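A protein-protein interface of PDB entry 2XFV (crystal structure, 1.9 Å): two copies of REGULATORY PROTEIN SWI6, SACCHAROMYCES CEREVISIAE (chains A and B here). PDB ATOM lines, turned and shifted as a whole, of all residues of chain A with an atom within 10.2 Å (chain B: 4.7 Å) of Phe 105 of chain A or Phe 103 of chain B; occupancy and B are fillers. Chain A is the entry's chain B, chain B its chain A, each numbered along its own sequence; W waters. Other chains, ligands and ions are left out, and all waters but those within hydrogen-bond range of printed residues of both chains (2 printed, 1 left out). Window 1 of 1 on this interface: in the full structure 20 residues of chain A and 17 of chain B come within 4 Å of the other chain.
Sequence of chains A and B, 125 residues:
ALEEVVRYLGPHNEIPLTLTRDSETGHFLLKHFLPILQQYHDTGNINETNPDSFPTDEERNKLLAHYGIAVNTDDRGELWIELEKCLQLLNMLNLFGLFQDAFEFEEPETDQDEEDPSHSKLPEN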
ATOM      1  N   GLU A   3     -10.322 -20.345  -9.593  1.00  0.00           N
ATOM      2  CA  GLU A   3      -9.023 -19.858  -9.127  1.00  0.00           C
ATOM      3  C   GLU A   3      -9.237 -18.370  -8.865  1.00  0.00           C
ATOM      4  O   GLU A   3      -9.867 -17.696  -9.671  1.00  0.00           O
ATOM      5  CB  GLU A   3      -7.982 -20.029 -10.232  1.00  0.00           C
ATOM      6  CG  GLU A   3      -6.680 -20.677  -9.805  1.00  0.00           C
ATOM      7  CD  GLU A   3      -5.575 -20.518 -10.846  1.00  0.00           C
ATOM      8  OE1 GLU A   3      -5.874 -20.121 -11.997  1.00  0.00           O
ATOM      9  OE2 GLU A   3      -4.402 -20.789 -10.503  1.00  0.00           O
ATOM     10  N   ARG A  21     -11.189 -16.786 -11.984  1.00  0.00           N
ATOM     11  CA  ARG A  21     -10.989 -17.466 -13.253  1.00  0.00           C
ATOM     12  C   ARG A  21     -11.522 -18.899 -13.197  1.00  0.00           C
ATOM     13  O   ARG A  21     -11.263 -19.625 -12.240  1.00  0.00           O
ATOM     14  CB  ARG A  21      -9.494 -17.444 -13.592  1.00  0.00           C
ATOM     15  CG  ARG A  21      -9.074 -18.221 -14.829  1.00  0.00           C
ATOM     16  CD  ARG A  21      -7.559 -18.441 -14.799  1.00  0.00           C
ATOM     17  NE  ARG A  21      -6.863 -17.713 -15.854  1.00  0.00           N
ATOM     18  CZ  ARG A  21      -5.555 -17.472 -15.863  1.00  0.00           C
ATOM     19  NH1 ARG A  21      -4.786 -17.879 -14.859  1.00  0.00           N
ATOM     20  NH2 ARG A  21      -5.018 -16.804 -16.871  1.00  0.00           N
ATOM     21  N   GLY A  26     -11.031 -20.888 -18.766  1.00  0.00           N
ATOM     22  CA  GLY A  26     -10.018 -19.845 -18.714  1.00  0.00           C
ATOM     23  C   GLY A  26     -10.565 -18.423 -18.653  1.00  0.00           C
ATOM     24  O   GLY A  26      -9.799 -17.456 -18.699  1.00  0.00           O
ATOM     25  N   PHE A  28     -12.799 -15.033 -17.059  1.00  0.00           N
ATOM     26  CA  PHE A  28     -12.845 -14.264 -15.808  1.00  0.00           C
ATOM     27  C   PHE A  28     -14.255 -13.759 -15.530  1.00  0.00           C
ATOM     28  O   PHE A  28     -14.959 -13.345 -16.456  1.00  0.00           O
ATOM     29  CB  PHE A  28     -11.891 -13.054 -15.883  1.00  0.00           C
ATOM     30  CG  PHE A  28     -10.433 -13.435 -15.917  1.00  0.00           C
ATOM     31  CD1 PHE A  28      -9.648 -13.339 -14.777  1.00  0.00           C
ATOM     32  CD2 PHE A  28      -9.852 -13.898 -17.088  1.00  0.00           C
ATOM     33  CE1 PHE A  28      -8.301 -13.701 -14.806  1.00  0.00           C
ATOM     34  CE2 PHE A  28      -8.517 -14.263 -17.129  1.00  0.00           C
ATOM     35  CZ  PHE A  28      -7.734 -14.166 -15.983  1.00  0.00           C
ATOM     36  N   LEU A  83      -9.526 -13.734 -21.324  1.00  0.00           N
ATOM     37  CA  LEU A  83      -8.266 -13.225 -20.807  1.00  0.00           C
ATOM     38  C   LEU A  83      -7.804 -11.957 -21.529  1.00  0.00           C
ATOM     39  O   LEU A  83      -7.374 -11.009 -20.896  1.00  0.00           O
ATOM     40  CB  LEU A  83      -7.180 -14.307 -20.929  1.00  0.00           C
ATOM     41  CG  LEU A  83      -5.758 -13.827 -20.619  1.00  0.00           C
ATOM     42  CD1 LEU A  83      -5.575 -13.511 -19.137  1.00  0.00           C
ATOM     43  CD2 LEU A  83      -4.735 -14.863 -21.072  1.00  0.00           C
ATOM     44  N   LEU A  87      -7.143  -8.362 -19.609  1.00  0.00           N
ATOM     45  CA  LEU A  87      -5.878  -7.622 -19.586  1.00  0.00           C
ATOM     46  C   LEU A  87      -6.037  -6.209 -20.144  1.00  0.00           C
ATOM     47  O   LEU A  87      -5.436  -5.260 -19.628  1.00  0.00           O
ATOM     48  CB  LEU A  87      -4.779  -8.358 -20.354  1.00  0.00           C
ATOM     49  CG  LEU A  87      -4.319  -9.671 -19.722  1.00  0.00           C
ATOM     50  CD1 LEU A  87      -3.444 -10.451 -20.704  1.00  0.00           C
ATOM     51  CD2 LEU A  87      -3.583  -9.395 -18.428  1.00  0.00           C
ATOM     52  N   PHE A  96      -2.679  -3.109 -13.951  1.00  0.00           N
ATOM     53  CA  PHE A  96      -1.823  -4.272 -14.179  1.00  0.00           C
ATOM     54  C   PHE A  96      -0.763  -4.358 -13.081  1.00  0.00           C
ATOM     55  O   PHE A  96      -0.475  -5.437 -12.573  1.00  0.00           O
ATOM     56  CB  PHE A  96      -1.160  -4.272 -15.553  1.00  0.00           C
ATOM     57  CG  PHE A  96      -0.328  -5.501 -15.801  1.00  0.00           C
ATOM     58  CD1 PHE A  96      -0.921  -6.676 -16.236  1.00  0.00           C
ATOM     59  CD2 PHE A  96       1.038  -5.495 -15.552  1.00  0.00           C
ATOM     60  CE1 PHE A  96      -0.166  -7.823 -16.441  1.00  0.00           C
ATOM     61  CE2 PHE A  96       1.799  -6.635 -15.760  1.00  0.00           C
ATOM     62  CZ  PHE A  96       1.196  -7.800 -16.200  1.00  0.00           C
ATOM     63  N   PHE A  99      -1.622  -6.182  -9.931  1.00  0.00           N
ATOM     64  CA  PHE A  99      -1.713  -7.636 -10.084  1.00  0.00           C
ATOM     65  C   PHE A  99      -0.421  -8.327 -10.550  1.00  0.00           C
ATOM     66  O   PHE A  99      -0.371  -9.552 -10.600  1.00  0.00           O
ATOM     67  CB  PHE A  99      -2.916  -8.019 -10.975  1.00  0.00           C
ATOM     68  CG  PHE A  99      -4.247  -7.786 -10.315  1.00  0.00           C
ATOM     69  CD1 PHE A  99      -4.825  -8.772  -9.534  1.00  0.00           C
ATOM     70  CD2 PHE A  99      -4.903  -6.570 -10.443  1.00  0.00           C
ATOM     71  CE1 PHE A  99      -6.035  -8.560  -8.906  1.00  0.00           C
ATOM     72  CE2 PHE A  99      -6.120  -6.348  -9.814  1.00  0.00           C
ATOM     73  CZ  PHE A  99      -6.688  -7.342  -9.039  1.00  0.00           C
ATOM     74  N   GLN A 100       0.622  -7.554 -10.865  1.00  0.00           N
ATOM     75  CA  GLN A 100       1.927  -8.113 -11.270  1.00  0.00           C
ATOM     76  C   GLN A 100       2.403  -9.191 -10.312  1.00  0.00           C
ATOM     77  O   GLN A 100       3.068 -10.155 -10.712  1.00  0.00           O
ATOM     78  CB  GLN A 100       3.026  -7.050 -11.191  1.00  0.00           C
ATOM     79  CG  GLN A 100       3.127  -6.066 -12.317  1.00  0.00           C
ATOM     80  CD  GLN A 100       4.086  -4.950 -11.958  1.00  0.00           C
ATOM     81  OE1 GLN A 100       4.115  -3.908 -12.608  1.00  0.00           O
ATOM     82  NE2 GLN A 100       4.869  -5.162 -10.897  1.00  0.00           N
ATOM     83  N   ASP A 101       2.125  -8.984  -9.032  1.00  0.00           N
ATOM     84  CA  ASP A 101       2.664  -9.861  -8.000  1.00  0.00           C
ATOM     85  C   ASP A 101       1.756 -11.065  -7.738  1.00  0.00           C
ATOM     86  O   ASP A 101       1.956 -11.777  -6.780  1.00  0.00           O
ATOM     87  CB  ASP A 101       2.964  -9.079  -6.699  1.00  0.00           C
ATOM     88  CG  ASP A 101       1.711  -8.551  -6.014  1.00  0.00           C
ATOM     89  OD1 ASP A 101       0.597  -8.812  -6.499  1.00  0.00           O
ATOM     90  OD2 ASP A 101       1.844  -7.865  -4.975  1.00  0.00           O
ATOM     91  N   ALA A 102       0.778 -11.296  -8.612  1.00  0.00           N
ATOM     92  CA  ALA A 102      -0.213 -12.354  -8.401  1.00  0.00           C
ATOM     93  C   ALA A 102       0.002 -13.612  -9.251  1.00  0.00           C
ATOM     94  O   ALA A 102      -0.722 -14.592  -9.079  1.00  0.00           O
ATOM     95  CB  ALA A 102      -1.642 -11.803  -8.626  1.00  0.00           C
ATOM     96  N   PHE A 103       0.988 -13.590 -10.151  1.00  0.00           N
ATOM     97  CA  PHE A 103       1.216 -14.702 -11.080  1.00  0.00           C
ATOM     98  C   PHE A 103       2.504 -15.475 -10.779  1.00  0.00           C
ATOM     99  O   PHE A 103       3.499 -14.897 -10.335  1.00  0.00           O
ATOM    100  CB  PHE A 103       1.250 -14.206 -12.535  1.00  0.00           C
ATOM    101  CG  PHE A 103      -0.066 -13.687 -13.028  1.00  0.00           C
ATOM    102  CD1 PHE A 103      -0.984 -14.542 -13.620  1.00  0.00           C
ATOM    103  CD2 PHE A 103      -0.395 -12.343 -12.887  1.00  0.00           C
ATOM    104  CE1 PHE A 103      -2.207 -14.070 -14.069  1.00  0.00           C
ATOM    105  CE2 PHE A 103      -1.616 -11.859 -13.332  1.00  0.00           C
ATOM    106  CZ  PHE A 103      -2.525 -12.726 -13.928  1.00  0.00           C
ATOM    107  N   GLU A 104       2.467 -16.783 -11.017  1.00  0.00           N
ATOM    108  CA  GLU A 104       3.646 -17.636 -10.866  1.00  0.00           C
ATOM    109  C   GLU A 104       3.848 -18.452 -12.145  1.00  0.00           C
ATOM    110  O   GLU A 104       2.878 -18.844 -12.810  1.00  0.00           O
ATOM    111  CB  GLU A 104       3.506 -18.566  -9.650  1.00  0.00           C
ATOM    112  CG  GLU A 104       3.484 -17.851  -8.287  1.00  0.00           C
ATOM    113  CD  GLU A 104       4.853 -17.318  -7.860  1.00  0.00           C
ATOM    114  OE1 GLU A 104       5.881 -17.864  -8.308  1.00  0.00           O
ATOM    115  OE2 GLU A 104       4.906 -16.358  -7.061  1.00  0.00           O
ATOM    116  N   PHE A 105       5.113 -18.690 -12.490  1.00  0.00           N
ATOM    117  CA  PHE A 105       5.465 -19.455 -13.682  1.00  0.00           C
ATOM    118  C   PHE A 105       5.169 -20.924 -13.441  1.00  0.00           C
ATOM    119  O   PHE A 105       5.476 -21.453 -12.379  1.00  0.00           O
ATOM    120  CB  PHE A 105       6.967 -19.283 -13.973  1.00  0.00           C
ATOM    121  CG  PHE A 105       7.436 -19.936 -15.262  1.00  0.00           C
ATOM    122  CD1 PHE A 105       7.264 -19.294 -16.489  1.00  0.00           C
ATOM    123  CD2 PHE A 105       8.089 -21.159 -15.240  1.00  0.00           C
ATOM    124  CE1 PHE A 105       7.718 -19.882 -17.668  1.00  0.00           C
ATOM    125  CE2 PHE A 105       8.538 -21.751 -16.412  1.00  0.00           C
ATOM    126  CZ  PHE A 105       8.359 -21.105 -17.625  1.00  0.00           C
ATOM    127  N   GLU A 106       4.580 -21.578 -14.434  1.00  0.00           N
ATOM    128  CA  GLU A 106       4.339 -23.016 -14.370  1.00  0.00           C
ATOM    129  C   GLU A 106       4.759 -23.629 -15.700  1.00  0.00           C
ATOM    130  O   GLU A 106       4.137 -23.367 -16.724  1.00  0.00           O
ATOM    131  CB  GLU A 106       2.853 -23.287 -14.114  1.00  0.00           C
ATOM    132  CG  GLU A 106       2.494 -24.744 -13.856  1.00  0.00           C
ATOM    133  CD  GLU A 106       2.789 -25.183 -12.430  1.00  0.00           C
ATOM    134  OE1 GLU A 106       3.800 -24.721 -11.856  1.00  0.00           O
ATOM    135  OE2 GLU A 106       2.010 -25.998 -11.885  1.00  0.00           O
ATOM    136  N   GLU A 107       5.824 -24.420 -15.701  1.00  0.00           N
ATOM    137  CA  GLU A 107       6.274 -25.059 -16.940  1.00  0.00           C
ATOM    138  C   GLU A 107       5.196 -25.996 -17.501  1.00  0.00           C
ATOM    139  O   GLU A 107       4.836 -26.984 -16.863  1.00  0.00           O
ATOM    140  CB  GLU A 107       7.587 -25.817 -16.713  1.00  0.00           C
ATOM    141  CG  GLU A 107       8.347 -26.140 -17.995  1.00  0.00           C
ATOM    142  CD  GLU A 107       9.647 -26.891 -17.736  1.00  0.00           C
ATOM    143  OE1 GLU A 107       9.752 -27.564 -16.687  1.00  0.00           O
ATOM    144  OE2 GLU A 107      10.562 -26.809 -18.586  1.00  0.00           O
ATOM    145  N   PRO A 108       4.664 -25.676 -18.693  1.00  0.00           N
ATOM    146  CA  PRO A 108       3.569 -26.446 -19.300  1.00  0.00           C
ATOM    147  C   PRO A 108       3.923 -27.913 -19.531  1.00  0.00           C
ATOM    148  O   PRO A 108       4.996 -28.188 -20.064  1.00  0.00           O
ATOM    149  CB  PRO A 108       3.347 -25.739 -20.640  1.00  0.00           C
ATOM    150  CG  PRO A 108       3.826 -24.343 -20.412  1.00  0.00           C
ATOM    151  CD  PRO A 108       4.999 -24.479 -19.485  1.00  0.00           C
ATOM    152  N   GLU B   3      14.080 -24.210 -16.352  1.00  0.00           N
ATOM    153  CA  GLU B   3      12.756 -24.541 -16.874  1.00  0.00           C
ATOM    154  C   GLU B   3      12.556 -23.640 -18.073  1.00  0.00           C
ATOM    155  O   GLU B   3      12.972 -22.485 -18.056  1.00  0.00           O
ATOM    156  CB  GLU B   3      11.679 -24.238 -15.822  1.00  0.00           C
ATOM    157  CG  GLU B   3      11.794 -25.107 -14.568  1.00  0.00           C
ATOM    158  CD  GLU B   3      10.938 -24.612 -13.399  1.00  0.00           C
ATOM    159  OE1 GLU B   3      10.272 -23.559 -13.511  1.00  0.00           O
ATOM    160  OE2 GLU B   3      10.942 -25.287 -12.355  1.00  0.00           O
ATOM    161  N   VAL B   5      10.098 -22.378 -21.681  1.00  0.00           N
ATOM    162  CA  VAL B   5       8.988 -22.416 -22.629  1.00  0.00           C
ATOM    163  C   VAL B   5       9.325 -21.484 -23.786  1.00  0.00           C
ATOM    164  O   VAL B   5       9.880 -20.405 -23.590  1.00  0.00           O
ATOM    165  CB  VAL B   5       7.645 -21.993 -21.981  1.00  0.00           C
ATOM    166  CG1 VAL B   5       7.749 -20.598 -21.397  1.00  0.00           C
ATOM    167  CG2 VAL B   5       6.514 -22.062 -22.999  1.00  0.00           C
ATOM    168  N   LEU B  19      11.342 -18.076 -22.705  1.00  0.00           N
ATOM    169  CA  LEU B  19      11.430 -17.804 -21.271  1.00  0.00           C
ATOM    170  C   LEU B  19      12.215 -18.935 -20.608  1.00  0.00           C
ATOM    171  O   LEU B  19      11.796 -20.090 -20.618  1.00  0.00           O
ATOM    172  CB  LEU B  19      10.042 -17.676 -20.636  1.00  0.00           C
ATOM    173  CG  LEU B  19       9.125 -16.634 -21.285  1.00  0.00           C
ATOM    174  CD1 LEU B  19       7.785 -16.528 -20.532  1.00  0.00           C
ATOM    175  CD2 LEU B  19       9.814 -15.264 -21.350  1.00  0.00           C
ATOM    176  N   ARG B  21      13.743 -19.965 -17.006  1.00  0.00           N
ATOM    177  CA  ARG B  21      13.685 -19.662 -15.569  1.00  0.00           C
ATOM    178  C   ARG B  21      14.652 -20.549 -14.765  1.00  0.00           C
ATOM    179  O   ARG B  21      14.743 -21.748 -15.016  1.00  0.00           O
ATOM    180  CB  ARG B  21      12.249 -19.869 -15.039  1.00  0.00           C
ATOM    181  CG  ARG B  21      11.963 -19.178 -13.685  1.00  0.00           C
ATOM    182  CD  ARG B  21      10.539 -19.471 -13.159  1.00  0.00           C
ATOM    183  NE  ARG B  21      10.488 -20.794 -12.548  1.00  0.00           N
ATOM    184  CZ  ARG B  21      10.502 -21.026 -11.238  1.00  0.00           C
ATOM    185  NH1 ARG B  21      10.480 -22.277 -10.790  1.00  0.00           N
ATOM    186  NH2 ARG B  21      10.536 -20.018 -10.374  1.00  0.00           N
ATOM    187  N   PHE B  28      14.617 -14.953 -14.684  1.00  0.00           N
ATOM    188  CA  PHE B  28      14.527 -15.323 -16.106  1.00  0.00           C
ATOM    189  C   PHE B  28      15.719 -14.761 -16.870  1.00  0.00           C
ATOM    190  O   PHE B  28      16.179 -13.668 -16.578  1.00  0.00           O
ATOM    191  CB  PHE B  28      13.239 -14.744 -16.722  1.00  0.00           C
ATOM    192  CG  PHE B  28      11.980 -15.399 -16.222  1.00  0.00           C
ATOM    193  CD1 PHE B  28      11.378 -16.413 -16.959  1.00  0.00           C
ATOM    194  CD2 PHE B  28      11.411 -15.012 -15.013  1.00  0.00           C
ATOM    195  CE1 PHE B  28      10.205 -17.020 -16.508  1.00  0.00           C
ATOM    196  CE2 PHE B  28      10.259 -15.622 -14.543  1.00  0.00           C
ATOM    197  CZ  PHE B  28       9.650 -16.623 -15.288  1.00  0.00           C
ATOM    198  N   LEU B  83      10.952 -12.076 -11.766  1.00  0.00           N
ATOM    199  CA  LEU B  83       9.648 -12.530 -12.259  1.00  0.00           C
ATOM    200  C   LEU B  83       8.722 -11.363 -12.579  1.00  0.00           C
ATOM    201  O   LEU B  83       8.056 -11.349 -13.612  1.00  0.00           O
ATOM    202  CB  LEU B  83       8.983 -13.423 -11.200  1.00  0.00           C
ATOM    203  CG  LEU B  83       7.489 -13.765 -11.330  1.00  0.00           C
ATOM    204  CD1 LEU B  83       7.215 -14.657 -12.544  1.00  0.00           C
ATOM    205  CD2 LEU B  83       6.985 -14.430 -10.048  1.00  0.00           C
ATOM    206  N   CYS B  86       9.758  -9.686 -15.723  1.00  0.00           N
ATOM    207  CA  CYS B  86       9.382 -10.524 -16.857  1.00  0.00           C
ATOM    208  C   CYS B  86       7.908 -10.293 -17.213  1.00  0.00           C
ATOM    209  O   CYS B  86       7.571 -10.072 -18.381  1.00  0.00           O
ATOM    210  CB  CYS B  86       9.654 -12.010 -16.560  1.00  0.00           C
ATOM    211  SG  CYS B  86       9.037 -13.158 -17.830  1.00  0.00           S
ATOM    212  N   LEU B  87       7.031 -10.306 -16.209  1.00  0.00           N
ATOM    213  CA  LEU B  87       5.602 -10.057 -16.466  1.00  0.00           C
ATOM    214  C   LEU B  87       5.347  -8.651 -17.032  1.00  0.00           C
ATOM    215  O   LEU B  87       4.553  -8.474 -17.966  1.00  0.00           O
ATOM    216  CB  LEU B  87       4.763 -10.299 -15.200  1.00  0.00           C
ATOM    217  CG  LEU B  87       4.709 -11.770 -14.753  1.00  0.00           C
ATOM    218  CD1 LEU B  87       4.412 -11.913 -13.255  1.00  0.00           C
ATOM    219  CD2 LEU B  87       3.690 -12.538 -15.583  1.00  0.00           C
ATOM    220  N   LEU B  90       6.346  -8.683 -20.767  1.00  0.00           N
ATOM    221  CA  LEU B  90       5.361  -9.382 -21.592  1.00  0.00           C
ATOM    222  C   LEU B  90       4.112  -8.528 -21.790  1.00  0.00           C
ATOM    223  O   LEU B  90       3.552  -8.463 -22.893  1.00  0.00           O
ATOM    224  CB  LEU B  90       4.983 -10.727 -20.970  1.00  0.00           C
ATOM    225  CG  LEU B  90       6.077 -11.786 -20.922  1.00  0.00           C
ATOM    226  CD1 LEU B  90       5.572 -12.982 -20.113  1.00  0.00           C
ATOM    227  CD2 LEU B  90       6.468 -12.201 -22.353  1.00  0.00           C
ATOM    228  N   PHE B  96       1.721 -11.275 -23.252  1.00  0.00           N
ATOM    229  CA  PHE B  96       1.286 -12.065 -22.107  1.00  0.00           C
ATOM    230  C   PHE B  96       0.268 -13.124 -22.527  1.00  0.00           C
ATOM    231  O   PHE B  96       0.308 -14.263 -22.050  1.00  0.00           O
ATOM    232  CB  PHE B  96       0.723 -11.215 -20.963  1.00  0.00           C
ATOM    233  CG  PHE B  96       0.382 -12.032 -19.750  1.00  0.00           C
ATOM    234  CD1 PHE B  96       1.376 -12.437 -18.875  1.00  0.00           C
ATOM    235  CD2 PHE B  96      -0.915 -12.470 -19.529  1.00  0.00           C
ATOM    236  CE1 PHE B  96       1.075 -13.214 -17.768  1.00  0.00           C
ATOM    237  CE2 PHE B  96      -1.224 -13.249 -18.426  1.00  0.00           C
ATOM    238  CZ  PHE B  96      -0.226 -13.619 -17.541  1.00  0.00           C
ATOM    239  N   PHE B  99       1.796 -16.282 -23.915  1.00  0.00           N
ATOM    240  CA  PHE B  99       2.363 -17.164 -22.892  1.00  0.00           C
ATOM    241  C   PHE B  99       1.402 -17.492 -21.742  1.00  0.00           C
ATOM    242  O   PHE B  99       1.839 -17.950 -20.687  1.00  0.00           O
ATOM    243  CB  PHE B  99       3.637 -16.549 -22.305  1.00  0.00           C
ATOM    244  CG  PHE B  99       4.817 -16.561 -23.245  1.00  0.00           C
ATOM    245  CD1 PHE B  99       5.747 -17.591 -23.201  1.00  0.00           C
ATOM    246  CD2 PHE B  99       5.006 -15.532 -24.160  1.00  0.00           C
ATOM    247  CE1 PHE B  99       6.834 -17.608 -24.065  1.00  0.00           C
ATOM    248  CE2 PHE B  99       6.092 -15.539 -25.028  1.00  0.00           C
ATOM    249  CZ  PHE B  99       7.008 -16.578 -24.980  1.00  0.00           C
ATOM    250  N   GLN B 100       0.103 -17.277 -21.944  1.00  0.00           N
ATOM    251  CA  GLN B 100      -0.873 -17.430 -20.856  1.00  0.00           C
ATOM    252  C   GLN B 100      -0.838 -18.788 -20.131  1.00  0.00           C
ATOM    253  O   GLN B 100      -1.001 -18.845 -18.912  1.00  0.00           O
ATOM    254  CB  GLN B 100      -2.299 -17.098 -21.333  1.00  0.00           C
ATOM    255  CG  GLN B 100      -2.899 -18.058 -22.374  1.00  0.00           C
ATOM    256  CD  GLN B 100      -4.156 -17.504 -23.065  1.00  0.00           C
ATOM    257  OE1 GLN B 100      -5.274 -17.656 -22.567  1.00  0.00           O
ATOM    258  NE2 GLN B 100      -3.971 -16.873 -24.226  1.00  0.00           N
ATOM    259  N   ASP B 101      -0.611 -19.872 -20.867  1.00  0.00           N
ATOM    260  CA  ASP B 101      -0.640 -21.198 -20.258  1.00  0.00           C
ATOM    261  C   ASP B 101       0.599 -21.488 -19.408  1.00  0.00           C
ATOM    262  O   ASP B 101       0.650 -22.503 -18.713  1.00  0.00           O
ATOM    263  CB  ASP B 101      -0.822 -22.290 -21.315  1.00  0.00           C
ATOM    264  CG  ASP B 101       0.373 -22.415 -22.237  1.00  0.00           C
ATOM    265  OD1 ASP B 101       1.113 -21.424 -22.387  1.00  0.00           O
ATOM    266  OD2 ASP B 101       0.574 -23.504 -22.814  1.00  0.00           O
ATOM    267  N   ALA B 102       1.589 -20.595 -19.457  1.00  0.00           N
ATOM    268  CA  ALA B 102       2.812 -20.753 -18.674  1.00  0.00           C
ATOM    269  C   ALA B 102       2.756 -20.024 -17.331  1.00  0.00           C
ATOM    270  O   ALA B 102       3.714 -20.067 -16.555  1.00  0.00           O
ATOM    271  CB  ALA B 102       4.033 -20.291 -19.481  1.00  0.00           C
ATOM    272  N   PHE B 103       1.643 -19.348 -17.070  1.00  0.00           N
ATOM    273  CA  PHE B 103       1.463 -18.584 -15.831  1.00  0.00           C
ATOM    274  C   PHE B 103       0.125 -18.918 -15.171  1.00  0.00           C
ATOM    275  O   PHE B 103      -0.893 -19.044 -15.849  1.00  0.00           O
ATOM    276  CB  PHE B 103       1.580 -17.078 -16.097  1.00  0.00           C
ATOM    277  CG  PHE B 103       2.976 -16.638 -16.467  1.00  0.00           C
ATOM    278  CD1 PHE B 103       3.918 -16.392 -15.480  1.00  0.00           C
ATOM    279  CD2 PHE B 103       3.349 -16.496 -17.801  1.00  0.00           C
ATOM    280  CE1 PHE B 103       5.216 -16.004 -15.810  1.00  0.00           C
ATOM    281  CE2 PHE B 103       4.640 -16.109 -18.149  1.00  0.00           C
ATOM    282  CZ  PHE B 103       5.580 -15.862 -17.150  1.00  0.00           C
ATOM    283  N   GLU B 104       0.140 -19.076 -13.851  1.00  0.00           N
ATOM    284  CA  GLU B 104      -1.077 -19.345 -13.087  1.00  0.00           C
ATOM    285  C   GLU B 104      -1.132 -18.405 -11.876  1.00  0.00           C
ATOM    286  O   GLU B 104      -0.146 -17.741 -11.557  1.00  0.00           O
ATOM    287  CB  GLU B 104      -1.095 -20.806 -12.628  1.00  0.00           C
ATOM    288  CG  GLU B 104      -0.001 -21.146 -11.622  1.00  0.00           C
ATOM    289  CD  GLU B 104      -0.009 -22.613 -11.196  1.00  0.00           C
ATOM    290  OE1 GLU B 104      -0.648 -23.439 -11.886  1.00  0.00           O
ATOM    291  OE2 GLU B 104       0.636 -22.938 -10.174  1.00  0.00           O
ATOM    292  N   PHE B 105      -2.282 -18.331 -11.211  1.00  0.00           N
ATOM    293  CA  PHE B 105      -2.405 -17.518  -9.996  1.00  0.00           C
ATOM    294  C   PHE B 105      -1.535 -18.082  -8.869  1.00  0.00           C
ATOM    295  O   PHE B 105      -1.419 -19.303  -8.714  1.00  0.00           O
ATOM    296  CB  PHE B 105      -3.852 -17.511  -9.501  1.00  0.00           C
ATOM    297  CG  PHE B 105      -4.784 -16.644 -10.314  1.00  0.00           C
ATOM    298  CD1 PHE B 105      -4.294 -15.711 -11.210  1.00  0.00           C
ATOM    299  CD2 PHE B 105      -6.159 -16.754 -10.150  1.00  0.00           C
ATOM    300  CE1 PHE B 105      -5.156 -14.918 -11.940  1.00  0.00           C
ATOM    301  CE2 PHE B 105      -7.025 -15.955 -10.876  1.00  0.00           C
ATOM    302  CZ  PHE B 105      -6.518 -15.046 -11.775  1.00  0.00           C
HETATM  303  O   HOH W   1      -2.454 -16.646 -17.432  1.00  0.00           O
HETATM  304  O   HOH W   2       7.455 -24.510 -12.967  1.00  0.00           O
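Arg 21 of chain A touches Phe 105 of chain B, and with the chains exchanged Phe 105 of chain A touches Arg 21 of chain B. Phe 103 of chain A touches Phe 105 of chain B, and with the chains exchanged Phe 105 of chain A touches Phe 103 of chain B. Of the 24 pairs that touch across the chains among the printed residues, 15 have their exchanged pair printed and touching as well.
Printed residues of chain B within 4 Å of Phe 105 of chain A: Glu 3 (3.7 Å), Val 5 (3.8 Å), Arg 21 (3.6 Å), Phe 28 (3.7 Å), Ala 102 (3.4 Å) and Phe 103 (3.9 Å). Of chain A, only Glu 104 (3.3 Å) and Phe 105 (3.9 Å) come within 4 Å of Phe 103 of chain B. Of chain A, only Phe 105 and Glu 107 come within 4 Å of Glu 3 of chain B. Of chain A, only Phe 105 (3.4 Å) and Glu 106 (2.7 Å) come within 4 Å of Ala 102 of chain B. Printed residues of chain B within 4 Å of Glu 104 of chain A: Phe 103 (3.3 Å) and Glu 104 (2.8 Å). Of the printed residues of chain B, Gln 100 of chain A touches Leu 87 (3.4 Å). Pro 108 of chain A touches none of the printed residues of chain B. The nearest printed residue of chain A that does not touch Phe 103 of chain B is Arg 21 of chain A (4.2 Å).
The side-chain carboxylate (OE1) of Glu 3 of chain B lies within salt-bridge range of the guanidinium group (NE) of Arg 21 of chain B, 2.9 Å away. N of Phe 96 of chain B is in hydrogen-bond range of O of Leu 90 of chain B (3.4 Å). NH1 of Arg 21 of chain A lies within salt-bridge range of OE1 of Glu 3 of chain A (3.8 Å).
Water W1 lies within hydrogen-bond range of NH2 of Arg 21 of chain A, O of Gln 100 of chain B and O of Phe 103 of chain B. Water W2 bridges the side-chain carboxylate (OE1) of Glu 3 of chain B (3.0 Å) and the backbone NH (N) of Glu 107 of chain A (3.2 Å).
Among the printed residues, pairs that only touch across the chains: Leu 83 of chain A with Gln 100 of chain B, Glu 104 of chain A with Phe 103 of chain B, Phe 103 of chain A with Glu 104 of chain B, Gln 100 of chain A with Leu 87 of chain B, Phe 105 of chain A with Ala 102 of chain B, Leu 87 of chain A with Phe 96 of chain B, Ala 102 of chain A with Phe 105 of chain B, Phe 103 of chain A with Leu 83 of chain B, Glu 107 of chain A with Glu 3 of chain B, Phe 105 of chain A with Arg 21 of chain B, Phe 105 of chain A with Glu 3 of chain B, Glu 106 of chain A with Glu 104 of chain B, Phe 105 of chain A with Phe 28 of chain B, Phe 103 of chain A with Phe 105 of chain B, Phe 28 of chain A with Phe 105 of chain B, Phe 105 of chain A with Val 5 of chain B, Phe 96 of chain A with Leu 87 of chain B, Phe 105 of chain A with Phe 103 of chain B, Glu 3 of chain A with Glu 104 of chain B, Arg 21 of chain A with Phe 105 of chain B and Phe 103 of chain A with Leu 87 of chain B.
The backbone NH (N) of Glu 106 of chain A lies within hydrogen-bond range of the backbone carbonyl oxygen (O) of Ala 102 of chain B, 2.7 Å away. N of Glu 104 of chain A sits at hydrogen-bond distance from O of Glu 104 of chain B (2.8 Å). The side-chain carboxylate (OE2) of Glu 3 of chain A lies within hydrogen-bond range of the backbone NH (N) of Phe 105 of chain B (3.3 Å).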
